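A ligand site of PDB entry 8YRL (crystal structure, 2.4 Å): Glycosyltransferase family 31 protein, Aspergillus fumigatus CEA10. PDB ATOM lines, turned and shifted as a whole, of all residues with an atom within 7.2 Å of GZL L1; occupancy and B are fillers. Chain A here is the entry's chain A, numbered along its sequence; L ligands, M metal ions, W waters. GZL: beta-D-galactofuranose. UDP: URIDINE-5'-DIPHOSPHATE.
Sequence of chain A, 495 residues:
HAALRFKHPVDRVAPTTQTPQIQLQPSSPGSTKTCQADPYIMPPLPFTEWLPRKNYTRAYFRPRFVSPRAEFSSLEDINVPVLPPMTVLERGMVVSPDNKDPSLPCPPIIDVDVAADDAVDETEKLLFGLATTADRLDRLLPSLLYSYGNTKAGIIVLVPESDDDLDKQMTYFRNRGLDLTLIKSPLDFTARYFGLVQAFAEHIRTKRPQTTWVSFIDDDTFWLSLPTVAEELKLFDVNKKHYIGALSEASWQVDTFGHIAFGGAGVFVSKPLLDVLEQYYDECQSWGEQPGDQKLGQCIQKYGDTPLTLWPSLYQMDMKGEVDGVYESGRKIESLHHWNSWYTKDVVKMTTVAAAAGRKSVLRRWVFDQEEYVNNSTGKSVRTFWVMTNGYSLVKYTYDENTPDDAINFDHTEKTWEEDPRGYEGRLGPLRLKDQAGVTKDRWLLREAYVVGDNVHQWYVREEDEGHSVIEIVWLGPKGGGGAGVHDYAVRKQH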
ATOM      1  N   ASP A 218      23.762 -24.617  -9.536  1.00  0.00           N
ATOM      2  CA  ASP A 218      23.786 -25.996  -9.090  1.00  0.00           C
ATOM      3  C   ASP A 218      24.541 -26.841 -10.108  1.00  0.00           C
ATOM      4  O   ASP A 218      24.713 -26.466 -11.258  1.00  0.00           O
ATOM      5  CB  ASP A 218      22.363 -26.537  -8.903  1.00  0.00           C
ATOM      6  CG  ASP A 218      21.751 -26.131  -7.581  1.00  0.00           C
ATOM      7  OD1 ASP A 218      22.091 -25.049  -7.059  1.00  0.00           O
ATOM      8  OD2 ASP A 218      20.919 -26.902  -7.057  1.00  0.00           O
ATOM      9  N   SER A 248      10.574 -19.622  -8.569  1.00  0.00           N
ATOM     10  CA  SER A 248      10.113 -20.990  -8.718  1.00  0.00           C
ATOM     11  C   SER A 248       8.747 -21.010  -9.410  1.00  0.00           C
ATOM     12  O   SER A 248       7.920 -20.115  -9.232  1.00  0.00           O
ATOM     13  CB  SER A 248      10.016 -21.663  -7.343  1.00  0.00           C
ATOM     14  OG  SER A 248       9.244 -22.854  -7.422  1.00  0.00           O
ATOM     15  N   GLN A 253       6.313 -22.222  -3.252  1.00  0.00           N
ATOM     16  CA  GLN A 253       7.746 -22.117  -2.992  1.00  0.00           C
ATOM     17  C   GLN A 253       8.168 -20.664  -2.868  1.00  0.00           C
ATOM     18  O   GLN A 253       9.029 -20.330  -2.052  1.00  0.00           O
ATOM     19  CB  GLN A 253       8.530 -22.823  -4.096  1.00  0.00           C
ATOM     20  CG  GLN A 253       8.213 -24.298  -4.247  1.00  0.00           C
ATOM     21  CD  GLN A 253       8.914 -25.175  -3.226  1.00  0.00           C
ATOM     22  OE1 GLN A 253       9.378 -24.694  -2.189  1.00  0.00           O
ATOM     23  NE2 GLN A 253       8.988 -26.476  -3.505  1.00  0.00           N
ATOM     24  N   VAL A 254       7.581 -19.782  -3.685  1.00  0.00           N
ATOM     25  CA  VAL A 254       7.822 -18.351  -3.535  1.00  0.00           C
ATOM     26  C   VAL A 254       7.255 -17.856  -2.206  1.00  0.00           C
ATOM     27  O   VAL A 254       7.880 -17.053  -1.509  1.00  0.00           O
ATOM     28  CB  VAL A 254       7.238 -17.580  -4.731  1.00  0.00           C
ATOM     29  CG1 VAL A 254       7.356 -16.082  -4.514  1.00  0.00           C
ATOM     30  CG2 VAL A 254       7.917 -18.005  -6.017  1.00  0.00           C
ATOM     31  N   THR A 256       6.974 -19.591   0.453  1.00  0.00           N
ATOM     32  CA  THR A 256       7.747 -20.163   1.556  1.00  0.00           C
ATOM     33  C   THR A 256       9.101 -19.481   1.702  1.00  0.00           C
ATOM     34  O   THR A 256       9.521 -19.182   2.829  1.00  0.00           O
ATOM     35  CB  THR A 256       7.935 -21.658   1.332  1.00  0.00           C
ATOM     36  OG1 THR A 256       6.659 -22.299   1.259  1.00  0.00           O
ATOM     37  CG2 THR A 256       8.734 -22.268   2.479  1.00  0.00           C
ATOM     38  N   PHE A 257       9.792 -19.208   0.602  1.00  0.00           N
ATOM     39  CA  PHE A 257      11.164 -18.722   0.646  1.00  0.00           C
ATOM     40  C   PHE A 257      11.327 -17.289   0.168  1.00  0.00           C
ATOM     41  O   PHE A 257      12.431 -16.741   0.274  1.00  0.00           O
ATOM     42  CB  PHE A 257      12.071 -19.647  -0.184  1.00  0.00           C
ATOM     43  CG  PHE A 257      12.060 -21.073   0.270  1.00  0.00           C
ATOM     44  CD1 PHE A 257      12.818 -21.475   1.360  1.00  0.00           C
ATOM     45  CD2 PHE A 257      11.280 -22.017  -0.382  1.00  0.00           C
ATOM     46  CE1 PHE A 257      12.806 -22.789   1.781  1.00  0.00           C
ATOM     47  CE2 PHE A 257      11.268 -23.330   0.039  1.00  0.00           C
ATOM     48  CZ  PHE A 257      12.027 -23.722   1.120  1.00  0.00           C
ATOM     49  N   ILE A 260      12.964 -14.585  -4.348  1.00  0.00           N
ATOM     50  CA  ILE A 260      14.400 -14.693  -4.484  1.00  0.00           C
ATOM     51  C   ILE A 260      14.720 -15.240  -5.879  1.00  0.00           C
ATOM     52  O   ILE A 260      13.842 -15.609  -6.649  1.00  0.00           O
ATOM     53  CB  ILE A 260      15.022 -15.587  -3.391  1.00  0.00           C
ATOM     54  CG1 ILE A 260      14.485 -17.019  -3.532  1.00  0.00           C
ATOM     55  CG2 ILE A 260      14.726 -15.025  -2.020  1.00  0.00           C
ATOM     56  CD1 ILE A 260      15.313 -18.049  -2.820  1.00  0.00           C
ATOM     57  N   ALA A 261      16.014 -15.287  -6.191  1.00  0.00           N
ATOM     58  CA  ALA A 261      16.503 -15.972  -7.377  1.00  0.00           C
ATOM     59  C   ALA A 261      16.813 -17.411  -6.988  1.00  0.00           C
ATOM     60  O   ALA A 261      17.809 -17.689  -6.326  1.00  0.00           O
ATOM     61  CB  ALA A 261      17.737 -15.272  -7.951  1.00  0.00           C
ATOM     62  N   PHE A 262      15.934 -18.328  -7.395  1.00  0.00           N
ATOM     63  CA  PHE A 262      16.097 -19.721  -7.028  1.00  0.00           C
ATOM     64  C   PHE A 262      17.326 -20.298  -7.714  1.00  0.00           C
ATOM     65  O   PHE A 262      17.449 -20.234  -8.949  1.00  0.00           O
ATOM     66  CB  PHE A 262      14.836 -20.503  -7.386  1.00  0.00           C
ATOM     67  CG  PHE A 262      13.711 -20.322  -6.403  1.00  0.00           C
ATOM     68  CD1 PHE A 262      13.035 -19.103  -6.331  1.00  0.00           C
ATOM     69  CD2 PHE A 262      13.337 -21.345  -5.545  1.00  0.00           C
ATOM     70  CE1 PHE A 262      12.011 -18.922  -5.416  1.00  0.00           C
ATOM     71  CE2 PHE A 262      12.317 -21.163  -4.640  1.00  0.00           C
ATOM     72  CZ  PHE A 262      11.644 -19.953  -4.578  1.00  0.00           C
ATOM     73  N   GLY A 263      18.233 -20.869  -6.919  1.00  0.00           N
ATOM     74  CA  GLY A 263      19.557 -21.211  -7.399  1.00  0.00           C
ATOM     75  C   GLY A 263      19.571 -22.278  -8.482  1.00  0.00           C
ATOM     76  O   GLY A 263      20.520 -22.354  -9.264  1.00  0.00           O
ATOM     77  N   GLY A 264      18.542 -23.119  -8.528  1.00  0.00           N
ATOM     78  CA  GLY A 264      18.511 -24.175  -9.529  1.00  0.00           C
ATOM     79  C   GLY A 264      18.467 -23.648 -10.949  1.00  0.00           C
ATOM     80  O   GLY A 264      19.108 -24.192 -11.851  1.00  0.00           O
ATOM     81  N   GLN A 290      20.228 -22.793   6.341  1.00  0.00           N
ATOM     82  CA  GLN A 290      19.398 -21.922   5.504  1.00  0.00           C
ATOM     83  C   GLN A 290      19.826 -22.093   4.049  1.00  0.00           C
ATOM     84  O   GLN A 290      21.024 -22.117   3.767  1.00  0.00           O
ATOM     85  CB  GLN A 290      19.511 -20.461   5.924  1.00  0.00           C
ATOM     86  CG  GLN A 290      19.050 -19.488   4.845  1.00  0.00           C
ATOM     87  CD  GLN A 290      18.911 -18.052   5.324  1.00  0.00           C
ATOM     88  OE1 GLN A 290      19.862 -17.471   5.839  1.00  0.00           O
ATOM     89  NE2 GLN A 290      17.724 -17.485   5.131  1.00  0.00           N
ATOM     90  N   PRO A 291      18.877 -22.237   3.122  1.00  0.00           N
ATOM     91  CA  PRO A 291      19.258 -22.376   1.709  1.00  0.00           C
ATOM     92  C   PRO A 291      20.111 -21.207   1.249  1.00  0.00           C
ATOM     93  O   PRO A 291      19.778 -20.043   1.486  1.00  0.00           O
ATOM     94  CB  PRO A 291      17.905 -22.424   0.987  1.00  0.00           C
ATOM     95  CG  PRO A 291      16.947 -22.925   2.016  1.00  0.00           C
ATOM     96  CD  PRO A 291      17.432 -22.356   3.322  1.00  0.00           C
ATOM     97  N   GLY A 292      21.229 -21.531   0.585  1.00  0.00           N
ATOM     98  CA  GLY A 292      22.166 -20.501   0.177  1.00  0.00           C
ATOM     99  C   GLY A 292      21.589 -19.501  -0.794  1.00  0.00           C
ATOM    100  O   GLY A 292      21.946 -18.321  -0.767  1.00  0.00           O
ATOM    101  N   ASP A 293      20.691 -19.951  -1.679  1.00  0.00           N
ATOM    102  CA  ASP A 293      20.089 -19.017  -2.631  1.00  0.00           C
ATOM    103  C   ASP A 293      19.136 -18.056  -1.932  1.00  0.00           C
ATOM    104  O   ASP A 293      19.018 -16.898  -2.356  1.00  0.00           O
ATOM    105  CB  ASP A 293      19.358 -19.798  -3.735  1.00  0.00           C
ATOM    106  CG  ASP A 293      18.357 -20.792  -3.185  1.00  0.00           C
ATOM    107  OD1 ASP A 293      18.297 -20.967  -1.953  1.00  0.00           O
ATOM    108  OD2 ASP A 293      17.614 -21.390  -4.001  1.00  0.00           O
ATOM    109  N   GLN A 294      18.439 -18.512  -0.888  1.00  0.00           N
ATOM    110  CA  GLN A 294      17.601 -17.603  -0.113  1.00  0.00           C
ATOM    111  C   GLN A 294      18.448 -16.642   0.712  1.00  0.00           C
ATOM    112  O   GLN A 294      18.126 -15.452   0.808  1.00  0.00           O
ATOM    113  CB  GLN A 294      16.661 -18.393   0.796  1.00  0.00           C
ATOM    114  CG  GLN A 294      15.582 -17.555   1.454  1.00  0.00           C
ATOM    115  CD  GLN A 294      14.953 -18.246   2.633  1.00  0.00           C
ATOM    116  OE1 GLN A 294      15.620 -18.950   3.390  1.00  0.00           O
ATOM    117  NE2 GLN A 294      13.653 -18.034   2.821  1.00  0.00           N
ATOM    118  N   LYS A 295      19.531 -17.147   1.307  1.00  0.00           N
ATOM    119  CA  LYS A 295      20.462 -16.269   2.023  1.00  0.00           C
ATOM    120  C   LYS A 295      21.063 -15.234   1.089  1.00  0.00           C
ATOM    121  O   LYS A 295      21.247 -14.074   1.474  1.00  0.00           O
ATOM    122  CB  LYS A 295      21.550 -17.100   2.690  1.00  0.00           C
ATOM    123  CG  LYS A 295      22.722 -16.276   3.204  1.00  0.00           C
ATOM    124  CD  LYS A 295      23.665 -17.116   4.030  1.00  0.00           C
ATOM    125  CE  LYS A 295      23.000 -17.521   5.324  1.00  0.00           C
ATOM    126  NZ  LYS A 295      22.875 -16.348   6.242  1.00  0.00           N
ATOM    127  N   GLN A 316      13.554 -23.211 -12.759  1.00  0.00           N
ATOM    128  CA  GLN A 316      13.963 -23.991 -11.607  1.00  0.00           C
ATOM    129  C   GLN A 316      13.420 -25.407 -11.655  1.00  0.00           C
ATOM    130  O   GLN A 316      14.070 -26.341 -11.167  1.00  0.00           O
ATOM    131  CB  GLN A 316      13.509 -23.282 -10.327  1.00  0.00           C
ATOM    132  CG  GLN A 316      13.444 -24.169  -9.094  1.00  0.00           C
ATOM    133  CD  GLN A 316      14.798 -24.343  -8.429  1.00  0.00           C
ATOM    134  OE1 GLN A 316      15.647 -23.460  -8.487  1.00  0.00           O
ATOM    135  NE2 GLN A 316      14.999 -25.503  -7.800  1.00  0.00           N
ATOM    136  N   ASP A 318      10.586 -26.719 -10.169  1.00  0.00           N
ATOM    137  CA  ASP A 318      10.098 -27.196  -8.867  1.00  0.00           C
ATOM    138  C   ASP A 318       8.826 -28.004  -9.085  1.00  0.00           C
ATOM    139  O   ASP A 318       7.716 -27.632  -8.684  1.00  0.00           O
ATOM    140  CB  ASP A 318       9.874 -26.031  -7.922  1.00  0.00           C
ATOM    141  CG  ASP A 318      11.126 -25.646  -7.150  1.00  0.00           C
ATOM    142  OD1 ASP A 318      12.073 -26.465  -7.117  1.00  0.00           O
ATOM    143  OD2 ASP A 318      11.166 -24.547  -6.578  1.00  0.00           O
ATOM    144  N   HIS A 337      16.673 -27.622 -14.855  1.00  0.00           N
ATOM    145  CA  HIS A 337      17.059 -28.016 -13.506  1.00  0.00           C
ATOM    146  C   HIS A 337      16.218 -29.212 -13.076  1.00  0.00           C
ATOM    147  O   HIS A 337      15.162 -29.485 -13.667  1.00  0.00           O
ATOM    148  CB  HIS A 337      16.899 -26.841 -12.534  1.00  0.00           C
ATOM    149  CG  HIS A 337      17.393 -27.124 -11.150  1.00  0.00           C
ATOM    150  ND1 HIS A 337      16.572 -27.075 -10.039  1.00  0.00           N
ATOM    151  CD2 HIS A 337      18.629 -27.456 -10.691  1.00  0.00           C
ATOM    152  CE1 HIS A 337      17.281 -27.364  -8.954  1.00  0.00           C
ATOM    153  NE2 HIS A 337      18.527 -27.601  -9.322  1.00  0.00           N
ATOM    154  N   HIS A 338      16.701 -29.915 -12.055  1.00  0.00           N
ATOM    155  CA  HIS A 338      16.015 -31.019 -11.394  1.00  0.00           C
ATOM    156  C   HIS A 338      15.818 -32.240 -12.293  1.00  0.00           C
ATOM    157  O   HIS A 338      15.073 -33.153 -11.932  1.00  0.00           O
ATOM    158  CB  HIS A 338      14.655 -30.594 -10.834  1.00  0.00           C
ATOM    159  CG  HIS A 338      14.727 -29.967  -9.471  1.00  0.00           C
ATOM    160  ND1 HIS A 338      13.815 -29.032  -9.033  1.00  0.00           N
ATOM    161  CD2 HIS A 338      15.604 -30.143  -8.460  1.00  0.00           C
ATOM    162  CE1 HIS A 338      14.124 -28.664  -7.805  1.00  0.00           C
ATOM    163  NE2 HIS A 338      15.207 -29.315  -7.437  1.00  0.00           N
ATOM    164  N   TRP A 342      14.376 -34.573  -8.972  1.00  0.00           N
ATOM    165  CA  TRP A 342      12.935 -34.435  -8.836  1.00  0.00           C
ATOM    166  C   TRP A 342      12.200 -35.155  -9.967  1.00  0.00           C
ATOM    167  O   TRP A 342      11.159 -35.782  -9.743  1.00  0.00           O
ATOM    168  CB  TRP A 342      12.548 -32.961  -8.797  1.00  0.00           C
ATOM    169  CG  TRP A 342      12.761 -32.318  -7.460  1.00  0.00           C
ATOM    170  CD1 TRP A 342      13.769 -32.579  -6.577  1.00  0.00           C
ATOM    171  CD2 TRP A 342      11.938 -31.322  -6.841  1.00  0.00           C
ATOM    172  NE1 TRP A 342      13.628 -31.810  -5.453  1.00  0.00           N
ATOM    173  CE2 TRP A 342      12.513 -31.029  -5.582  1.00  0.00           C
ATOM    174  CE3 TRP A 342      10.781 -30.643  -7.225  1.00  0.00           C
ATOM    175  CZ2 TRP A 342      11.959 -30.083  -4.714  1.00  0.00           C
ATOM    176  CZ3 TRP A 342      10.230 -29.717  -6.357  1.00  0.00           C
ATOM    177  CH2 TRP A 342      10.825 -29.440  -5.126  1.00  0.00           C
HETATM  178  C6  GZL L   1      15.452 -22.747  -1.328  1.00  0.00           C
HETATM  179  C5  GZL L   1      15.054 -23.228  -2.741  1.00  0.00           C
HETATM  180  C4  GZL L   1      14.050 -24.396  -2.546  1.00  0.00           C
HETATM  181  C3  GZL L   1      13.860 -25.156  -3.896  1.00  0.00           C
HETATM  182  C2  GZL L   1      14.041 -26.639  -3.459  1.00  0.00           C
HETATM  183  O6  GZL L   1      15.803 -21.413  -1.416  1.00  0.00           O
HETATM  184  O5  GZL L   1      16.180 -23.753  -3.386  1.00  0.00           O
HETATM  185  O4  GZL L   1      14.542 -25.309  -1.589  1.00  0.00           O
HETATM  186  O3  GZL L   1      12.558 -24.908  -4.326  1.00  0.00           O
HETATM  187  C1  GZL L   1      13.975 -26.549  -1.900  1.00  0.00           C
HETATM  188  O2  GZL L   1      15.344 -26.988  -3.811  1.00  0.00           O
HETATM  189  O1  GZL L   1      12.653 -26.467  -1.541  1.00  0.00           O
HETATM  190  N1  UDP L   2      24.063 -30.746  -4.273  1.00  0.00           N
HETATM  191  C2  UDP L   2      25.415 -30.435  -4.277  1.00  0.00           C
HETATM  192  N3  UDP L   2      25.784 -29.483  -5.193  1.00  0.00           N
HETATM  193  C4  UDP L   2      24.956 -28.833  -6.096  1.00  0.00           C
HETATM  194  C5  UDP L   2      23.581 -29.221  -6.031  1.00  0.00           C
HETATM  195  C6  UDP L   2      23.192 -30.146  -5.140  1.00  0.00           C
HETATM  196  O2  UDP L   2      26.216 -30.954  -3.515  1.00  0.00           O
HETATM  197  O4  UDP L   2      25.446 -27.995  -6.876  1.00  0.00           O
HETATM  198  C1' UDP L   2      23.607 -31.756  -3.311  1.00  0.00           C
HETATM  199  C2' UDP L   2      23.088 -31.151  -1.993  1.00  0.00           C
HETATM  200  O2' UDP L   2      23.408 -31.996  -0.899  1.00  0.00           O
HETATM  201  C3' UDP L   2      21.575 -31.097  -2.251  1.00  0.00           C
HETATM  202  C4' UDP L   2      21.354 -32.364  -3.066  1.00  0.00           C
HETATM  203  O4' UDP L   2      22.532 -32.479  -3.897  1.00  0.00           O
HETATM  204  O3' UDP L   2      20.827 -31.129  -1.045  1.00  0.00           O
HETATM  205  C5' UDP L   2      20.112 -32.358  -3.932  1.00  0.00           C
HETATM  206  O5' UDP L   2      20.168 -31.238  -4.841  1.00  0.00           O
HETATM  207  PA  UDP L   2      19.291 -31.216  -6.153  1.00  0.00           P
HETATM  208  O1A UDP L   2      19.945 -30.283  -7.102  1.00  0.00           O
HETATM  209  O2A UDP L   2      19.012 -32.624  -6.651  1.00  0.00           O
HETATM  210  O3A UDP L   2      17.888 -30.623  -5.695  1.00  0.00           O
HETATM  211  PB  UDP L   2      17.695 -29.181  -5.053  1.00  0.00           P
HETATM  212  O1B UDP L   2      18.344 -29.070  -3.717  1.00  0.00           O
HETATM  213  O2B UDP L   2      16.175 -29.024  -5.028  1.00  0.00           O
HETATM  214  O3B UDP L   2      18.287 -28.256  -6.122  1.00  0.00           O
HETATM  215 MN    MN M   1      19.835 -28.582  -8.033  1.00  0.00          MN
HETATM  216  O   HOH W   1      13.741 -29.714  -1.343  1.00  0.00           O
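An oxygen (O3) of GZL L1 is in hydrogen-bond range of the side-chain carboxylate (OD2) of Asp 318, 2.7 Å away. The side-chain carboxylate (OD1) of Asp 293 is in hydrogen-bond range of an oxygen (O6) of GZL L1 (2.6 Å). O2B of UDP L2 lies within hydrogen-bond range of NE2 of His 338 (2.6 Å).
An oxygen (O2) of GZL L1 sits at hydrogen-bond distance from an oxygen (O2B) of UDP L2 (2.5 Å).
The side-chain carboxylate (OD2) of Asp 293 lies within hydrogen-bond range of the backbone NH (N) of Gly 263 (3.0 Å). The side-chain carboxylate of Asp 318 lies within hydrogen-bond range of the side-chain hydroxyl of Ser 248 (2.7 Å). The side-chain carboxylate (OD1) of Asp 318 sits at hydrogen-bond distance from the side-chain amide nitrogen (NE2) of Gln 316 (3.2 Å). The backbone carbonyl oxygen of Phe 257 is in hydrogen-bond range of the side-chain amide nitrogen of Gln 294, 3.1 Å away. OE1 of Gln 294 lies within hydrogen-bond range of NE2 of Gln 290 (3.1 Å).
Gln 253 touches GZL L1 (OE1 to O1, 3.8 Å). Phe 257 touches GZL L1. CD1 of Ile 260 touches O6 of GZL L1 (3.7 Å). CE2 of Phe 262 touches O3 of GZL L1 (3.8 Å). CB of Pro 291 touches O6 of GZL L1, 3.3 Å away. CB of Gln 294 touches O6 of GZL L1 (3.8 Å). Hydrophobic or aromatic side chains within 4 Å of GZL L1: Phe 257, Ile 260, Phe 262 and Pro 291. Eight residues have an atom within 4 Å of GZL L1: Gln 253, Phe 257, Ile 260, Phe 262, Pro 291, Asp 293, Gln 294 and Asp 318. The nearest printed residue that does not touch GZL L1 is Gln 316 (4.1 Å).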
